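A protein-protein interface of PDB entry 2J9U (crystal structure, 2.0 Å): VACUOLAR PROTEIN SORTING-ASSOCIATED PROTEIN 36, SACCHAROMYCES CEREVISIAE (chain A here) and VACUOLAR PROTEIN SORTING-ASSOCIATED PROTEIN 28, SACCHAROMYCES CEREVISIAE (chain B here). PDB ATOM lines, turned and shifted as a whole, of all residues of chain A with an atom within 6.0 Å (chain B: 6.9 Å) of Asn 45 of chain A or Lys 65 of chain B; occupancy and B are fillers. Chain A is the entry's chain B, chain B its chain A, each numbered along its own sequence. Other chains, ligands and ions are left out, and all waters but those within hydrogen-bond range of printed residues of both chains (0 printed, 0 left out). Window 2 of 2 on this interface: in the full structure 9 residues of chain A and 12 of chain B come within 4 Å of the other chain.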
ATOM      1  N   CYS A  23       3.501  16.777  11.755  1.00  0.00           N
ATOM      2  CA  CYS A  23       2.731  16.350  12.925  1.00  0.00           C
ATOM      3  C   CYS A  23       3.291  16.820  14.278  1.00  0.00           C
ATOM      4  O   CYS A  23       2.614  16.689  15.300  1.00  0.00           O
ATOM      5  CB  CYS A  23       2.553  14.834  12.927  1.00  0.00           C
ATOM      6  SG  CYS A  23       4.043  13.852  13.297  1.00  0.00           S
ATOM      7  N   VAL A  25       5.834  15.736  16.146  1.00  0.00           N
ATOM      8  CA  VAL A  25       6.456  14.790  17.069  1.00  0.00           C
ATOM      9  C   VAL A  25       7.982  14.793  16.947  1.00  0.00           C
ATOM     10  O   VAL A  25       8.522  14.973  15.868  1.00  0.00           O
ATOM     11  CB  VAL A  25       5.848  13.312  17.096  1.00  0.00           C
ATOM     12  CG1 VAL A  25       4.342  13.232  16.804  1.00  0.00           C
ATOM     13  CG2 VAL A  25       6.706  12.279  16.391  1.00  0.00           C
ATOM     14  N   ASN A  27      11.602  13.342  16.636  1.00  0.00           N
ATOM     15  CA  ASN A  27      12.266  12.158  16.090  1.00  0.00           C
ATOM     16  C   ASN A  27      13.785  12.159  16.410  1.00  0.00           C
ATOM     17  O   ASN A  27      14.383  13.229  16.698  1.00  0.00           O
ATOM     18  CB  ASN A  27      12.070  12.112  14.584  1.00  0.00           C
ATOM     19  CG  ASN A  27      10.682  11.597  14.159  1.00  0.00           C
ATOM     20  OD1 ASN A  27      10.569  10.425  13.791  1.00  0.00           O
ATOM     21  ND2 ASN A  27       9.650  12.482  14.140  1.00  0.00           N
ATOM     22  N   CYS A  43       9.540  10.388   9.495  1.00  0.00           N
ATOM     23  CA  CYS A  43       8.885  10.475  10.794  1.00  0.00           C
ATOM     24  C   CYS A  43       8.250   9.135  11.237  1.00  0.00           C
ATOM     25  O   CYS A  43       7.479   8.528  10.490  1.00  0.00           O
ATOM     26  CB  CYS A  43       7.812  11.568  10.784  1.00  0.00           C
ATOM     27  SG  CYS A  43       6.845  11.783  12.311  1.00  0.00           S
ATOM     28  N   ILE A  44       8.552   8.727  12.466  1.00  0.00           N
ATOM     29  CA  ILE A  44       7.990   7.485  13.037  1.00  0.00           C
ATOM     30  C   ILE A  44       6.435   7.483  13.196  1.00  0.00           C
ATOM     31  O   ILE A  44       5.815   6.421  13.246  1.00  0.00           O
ATOM     32  CB  ILE A  44       8.681   7.133  14.378  1.00  0.00           C
ATOM     33  CG1 ILE A  44       8.377   5.688  14.780  1.00  0.00           C
ATOM     34  CG2 ILE A  44       8.272   8.079  15.476  1.00  0.00           C
ATOM     35  CD1 ILE A  44       9.566   4.745  14.591  1.00  0.00           C
ATOM     36  N   ASN A  45       5.834   8.676  13.244  1.00  0.00           N
ATOM     37  CA  ASN A  45       4.416   8.801  13.568  1.00  0.00           C
ATOM     38  C   ASN A  45       3.550   8.944  12.301  1.00  0.00           C
ATOM     39  O   ASN A  45       2.592   8.182  12.129  1.00  0.00           O
ATOM     40  CB  ASN A  45       4.199   9.984  14.529  1.00  0.00           C
ATOM     41  CG  ASN A  45       2.729  10.189  14.893  1.00  0.00           C
ATOM     42  OD1 ASN A  45       2.095   9.288  15.451  1.00  0.00           O
ATOM     43  ND2 ASN A  45       2.197  11.382  14.609  1.00  0.00           N
ATOM     44  N   CYS A  46       3.876   9.894  11.415  1.00  0.00           N
ATOM     45  CA  CYS A  46       3.009  10.146  10.234  1.00  0.00           C
ATOM     46  C   CYS A  46       3.630   9.537   8.983  1.00  0.00           C
ATOM     47  O   CYS A  46       2.981   9.426   7.937  1.00  0.00           O
ATOM     48  CB  CYS A  46       2.780  11.671  10.042  1.00  0.00           C
ATOM     49  SG  CYS A  46       4.298  12.576   9.561  1.00  0.00           S
ATOM     50  N   GLY A  47       4.877   9.075   9.105  1.00  0.00           N
ATOM     51  CA  GLY A  47       5.583   8.461   7.985  1.00  0.00           C
ATOM     52  C   GLY A  47       5.923   9.366   6.796  1.00  0.00           C
ATOM     53  O   GLY A  47       6.243   8.878   5.726  1.00  0.00           O
ATOM     54  N   LYS B  28      -3.513   2.338   1.533  1.00  0.00           N
ATOM     55  CA  LYS B  28      -2.447   3.052   2.216  1.00  0.00           C
ATOM     56  C   LYS B  28      -1.370   3.482   1.224  1.00  0.00           C
ATOM     57  O   LYS B  28      -0.949   4.618   1.235  1.00  0.00           O
ATOM     58  CB  LYS B  28      -1.825   2.185   3.358  1.00  0.00           C
ATOM     59  CG  LYS B  28      -0.519   2.734   3.977  1.00  0.00           C
ATOM     60  CD  LYS B  28       0.040   1.798   5.056  1.00  0.00           C
ATOM     61  CE  LYS B  28       1.212   2.425   5.774  1.00  0.00           C
ATOM     62  NZ  LYS B  28       1.753   1.463   6.769  1.00  0.00           N
ATOM     63  N   HIS B  32      -1.250   7.564   0.975  1.00  0.00           N
ATOM     64  CA  HIS B  32      -0.239   8.161   1.874  1.00  0.00           C
ATOM     65  C   HIS B  32       0.705   9.162   1.153  1.00  0.00           C
ATOM     66  O   HIS B  32       0.905  10.291   1.639  1.00  0.00           O
ATOM     67  CB  HIS B  32       0.540   7.118   2.678  1.00  0.00           C
ATOM     68  CG  HIS B  32       1.415   7.709   3.760  1.00  0.00           C
ATOM     69  ND1 HIS B  32       2.725   8.077   3.541  1.00  0.00           N
ATOM     70  CD2 HIS B  32       1.178   7.946   5.074  1.00  0.00           C
ATOM     71  CE1 HIS B  32       3.237   8.561   4.654  1.00  0.00           C
ATOM     72  NE2 HIS B  32       2.317   8.491   5.598  1.00  0.00           N
ATOM     73  N   ILE B  57      -3.948  16.278   9.068  1.00  0.00           N
ATOM     74  CA  ILE B  57      -2.880  15.634   9.869  1.00  0.00           C
ATOM     75  C   ILE B  57      -3.340  14.292  10.520  1.00  0.00           C
ATOM     76  O   ILE B  57      -2.643  13.257  10.396  1.00  0.00           O
ATOM     77  CB  ILE B  57      -2.221  16.600  10.883  1.00  0.00           C
ATOM     78  CG1 ILE B  57      -1.601  17.805  10.129  1.00  0.00           C
ATOM     79  CG2 ILE B  57      -1.086  15.862  11.689  1.00  0.00           C
ATOM     80  CD1 ILE B  57      -1.335  19.079  10.973  1.00  0.00           C
ATOM     81  N   TRP B  59      -5.696  12.354   9.546  1.00  0.00           N
ATOM     82  CA  TRP B  59      -5.892  11.344   8.495  1.00  0.00           C
ATOM     83  C   TRP B  59      -4.576  10.698   8.051  1.00  0.00           C
ATOM     84  O   TRP B  59      -4.496   9.480   7.923  1.00  0.00           O
ATOM     85  CB  TRP B  59      -6.592  11.945   7.302  1.00  0.00           C
ATOM     86  CG  TRP B  59      -8.112  11.945   7.374  1.00  0.00           C
ATOM     87  CD1 TRP B  59      -8.926  13.051   7.459  1.00  0.00           C
ATOM     88  CD2 TRP B  59      -8.984  10.818   7.212  1.00  0.00           C
ATOM     89  NE1 TRP B  59     -10.244  12.681   7.388  1.00  0.00           N
ATOM     90  CE2 TRP B  59     -10.320  11.318   7.252  1.00  0.00           C
ATOM     91  CE3 TRP B  59      -8.776   9.429   7.076  1.00  0.00           C
ATOM     92  CZ2 TRP B  59     -11.444  10.485   7.168  1.00  0.00           C
ATOM     93  CZ3 TRP B  59      -9.904   8.592   6.982  1.00  0.00           C
ATOM     94  CH2 TRP B  59     -11.219   9.118   7.046  1.00  0.00           C
ATOM     95  N   ILE B  60      -3.531  11.499   7.812  1.00  0.00           N
ATOM     96  CA  ILE B  60      -2.300  10.879   7.361  1.00  0.00           C
ATOM     97  C   ILE B  60      -1.639   9.979   8.475  1.00  0.00           C
ATOM     98  O   ILE B  60      -1.103   8.920   8.153  1.00  0.00           O
ATOM     99  CB  ILE B  60      -1.318  11.881   6.735  1.00  0.00           C
ATOM    100  CG1 ILE B  60      -0.321  11.066   5.866  1.00  0.00           C
ATOM    101  CG2 ILE B  60      -0.604  12.645   7.860  1.00  0.00           C
ATOM    102  CD1 ILE B  60       0.690  11.819   5.137  1.00  0.00           C
ATOM    103  N   VAL B  61      -1.762  10.380   9.753  1.00  0.00           N
ATOM    104  CA  VAL B  61      -1.367   9.550  10.924  1.00  0.00           C
ATOM    105  C   VAL B  61      -2.160   8.202  10.985  1.00  0.00           C
ATOM    106  O   VAL B  61      -1.567   7.099  11.114  1.00  0.00           O
ATOM    107  CB  VAL B  61      -1.456  10.347  12.287  1.00  0.00           C
ATOM    108  CG1 VAL B  61      -1.155   9.441  13.536  1.00  0.00           C
ATOM    109  CG2 VAL B  61      -0.512  11.590  12.275  1.00  0.00           C
ATOM    110  N   ARG B  62      -3.478   8.296  10.850  1.00  0.00           N
ATOM    111  CA  ARG B  62      -4.356   7.132  10.782  1.00  0.00           C
ATOM    112  C   ARG B  62      -4.005   6.202   9.605  1.00  0.00           C
ATOM    113  O   ARG B  62      -3.877   4.965   9.763  1.00  0.00           O
ATOM    114  CB  ARG B  62      -5.817   7.597  10.723  1.00  0.00           C
ATOM    115  CG  ARG B  62      -6.469   7.796  12.095  1.00  0.00           C
ATOM    116  CD  ARG B  62      -8.019   7.806  12.000  1.00  0.00           C
ATOM    117  NE  ARG B  62      -8.524   9.063  11.507  1.00  0.00           N
ATOM    118  CZ  ARG B  62      -9.720   9.346  10.992  1.00  0.00           C
ATOM    119  NH1 ARG B  62     -10.699   8.452  10.827  1.00  0.00           N
ATOM    120  NH2 ARG B  62      -9.910  10.599  10.623  1.00  0.00           N
ATOM    121  N   ILE B  63      -3.782   6.795   8.427  1.00  0.00           N
ATOM    122  CA  ILE B  63      -3.441   5.998   7.217  1.00  0.00           C
ATOM    123  C   ILE B  63      -2.059   5.338   7.342  1.00  0.00           C
ATOM    124  O   ILE B  63      -1.871   4.165   6.922  1.00  0.00           O
ATOM    125  CB  ILE B  63      -3.598   6.842   5.899  1.00  0.00           C
ATOM    126  CG1 ILE B  63      -5.067   7.134   5.597  1.00  0.00           C
ATOM    127  CG2 ILE B  63      -2.944   6.165   4.687  1.00  0.00           C
ATOM    128  CD1 ILE B  63      -5.309   8.247   4.542  1.00  0.00           C
ATOM    129  N   ASN B  64      -1.107   6.050   7.938  1.00  0.00           N
ATOM    130  CA  ASN B  64       0.206   5.460   8.252  1.00  0.00           C
ATOM    131  C   ASN B  64       0.189   4.182   9.134  1.00  0.00           C
ATOM    132  O   ASN B  64       1.101   3.337   9.020  1.00  0.00           O
ATOM    133  CB  ASN B  64       1.127   6.489   8.878  1.00  0.00           C
ATOM    134  CG  ASN B  64       2.558   6.068   8.831  1.00  0.00           C
ATOM    135  OD1 ASN B  64       3.079   5.734   7.764  1.00  0.00           O
ATOM    136  ND2 ASN B  64       3.219   6.080   9.987  1.00  0.00           N
ATOM    137  N   LYS B  65      -0.818   4.056  10.009  1.00  0.00           N
ATOM    138  CA  LYS B  65      -0.911   2.925  10.955  1.00  0.00           C
ATOM    139  C   LYS B  65      -1.577   1.701  10.348  1.00  0.00           C
ATOM    140  O   LYS B  65      -1.622   0.632  10.968  1.00  0.00           O
ATOM    141  CB  LYS B  65      -1.640   3.339  12.234  1.00  0.00           C
ATOM    142  CG  LYS B  65      -0.804   4.240  13.120  1.00  0.00           C
ATOM    143  CD  LYS B  65      -1.637   4.903  14.220  1.00  0.00           C
ATOM    144  CE  LYS B  65      -0.861   6.031  14.932  1.00  0.00           C
ATOM    145  NZ  LYS B  65       0.639   5.936  14.835  1.00  0.00           N
ATOM    146  N   LEU B  66      -2.114   1.848   9.140  1.00  0.00           N
ATOM    147  CA  LEU B  66      -2.718   0.694   8.465  1.00  0.00           C
ATOM    148  C   LEU B  66      -1.663  -0.361   8.098  1.00  0.00           C
ATOM    149  O   LEU B  66      -0.487  -0.038   7.938  1.00  0.00           O
ATOM    150  CB  LEU B  66      -3.478   1.129   7.207  1.00  0.00           C
ATOM    151  CG  LEU B  66      -4.716   2.033   7.280  1.00  0.00           C
ATOM    152  CD1 LEU B  66      -5.099   2.431   5.883  1.00  0.00           C
ATOM    153  CD2 LEU B  66      -5.896   1.371   7.993  1.00  0.00           C
ATOM    154  N   SER B  67      -2.086  -1.617   7.971  1.00  0.00           N
ATOM    155  CA  SER B  67      -1.199  -2.696   7.516  1.00  0.00           C
ATOM    156  C   SER B  67      -1.145  -2.707   6.000  1.00  0.00           C
ATOM    157  O   SER B  67      -2.017  -2.134   5.338  1.00  0.00           O
ATOM    158  CB  SER B  67      -1.676  -4.059   8.026  1.00  0.00           C
ATOM    159  OG  SER B  67      -1.841  -4.010   9.431  1.00  0.00           O
ATOM    160  N   ASP B  70      -4.393  -2.844   3.575  1.00  0.00           N
ATOM    161  CA  ASP B  70      -5.654  -2.393   4.144  1.00  0.00           C
ATOM    162  C   ASP B  70      -6.200  -1.295   3.240  1.00  0.00           C
ATOM    163  O   ASP B  70      -5.438  -0.545   2.611  1.00  0.00           O
ATOM    164  CB  ASP B  70      -5.486  -1.804   5.554  1.00  0.00           C
ATOM    165  CG  ASP B  70      -5.154  -2.845   6.619  1.00  0.00           C
ATOM    166  OD1 ASP B  70      -4.916  -2.434   7.784  1.00  0.00           O
ATOM    167  OD2 ASP B  70      -5.121  -4.055   6.300  1.00  0.00           O
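O of Cys 46 of chain A lies within hydrogen-bond range of NE2 of His 32 of chain B (2.6 Å).
The side-chain amide nitrogen (ND2) of Asn 64 of chain B is in hydrogen-bond range of the backbone carbonyl oxygen (O) of Asn 45 of chain A.
NZ of Lys 28 of chain B lies within hydrogen-bond range of O of Asn 64 of chain B, 3.0 Å away.
SG of Cys 23 of chain A lies close to ND2 of Asn 45 of chain A (3.4 Å).
The side-chain sulfur (SG) of Cys 43 of chain A sits close to the backbone NH (N) of Asn 45 of chain A, 3.4 Å away.
Cys 23 of chain A touches Ile 57 of chain B (CB to CG2, 3.98 Å).
CG2 of Val 61 of chain B touches ND2 of Asn 45 of chain A, at 3.6 Å.
Asn 45 of chain A touches Lys 65 of chain B (OD1 to NZ, 3.7 Å).
CG2 of Val 61 of chain B touches CB of Cys 46 of chain A, at 3.98 Å.
Cys 46 of chain A touches Asn 64 of chain B.
O of Gly 47 of chain A touches CE1 of His 32 of chain B, at 3.2 Å.
Gly 47 of chain A touches Asn 64 of chain B.
Of chain B, only Val 61 (3.6 Å), Asn 64 (3.1 Å) and Lys 65 (3.7 Å) come within 4 Å of Asn 45 of chain A.
Of chain A, only Asn 45 (3.7 Å) comes within 4 Å of Lys 65 of chain B.
Printed residues of chain B within 4 Å of Cys 46 of chain A: His 32, Val 61 and Asn 64.
Of the printed residues of chain B, Cys 23 of chain A touches Ile 57 (3.98 Å).
Trp 59 of chain B touches none of the printed residues of chain A.
The nearest residue of chain B that does not touch Asn 45 of chain A is Ile 60 of chain B (5.5 Å).
The nearest printed residue of chain B that does not touch Cys 46 of chain A is Ile 60 of chain B (4.1 Å).
Of the 13 printed residues of chain B, 5 touch a printed residue of chain A.
Printed residues of chain B that touch a printed residue of chain A: His 32, Ile 57, Val 61, Asn 64 and Lys 65.
Among the printed residues, 9 pairs touch across the chains.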
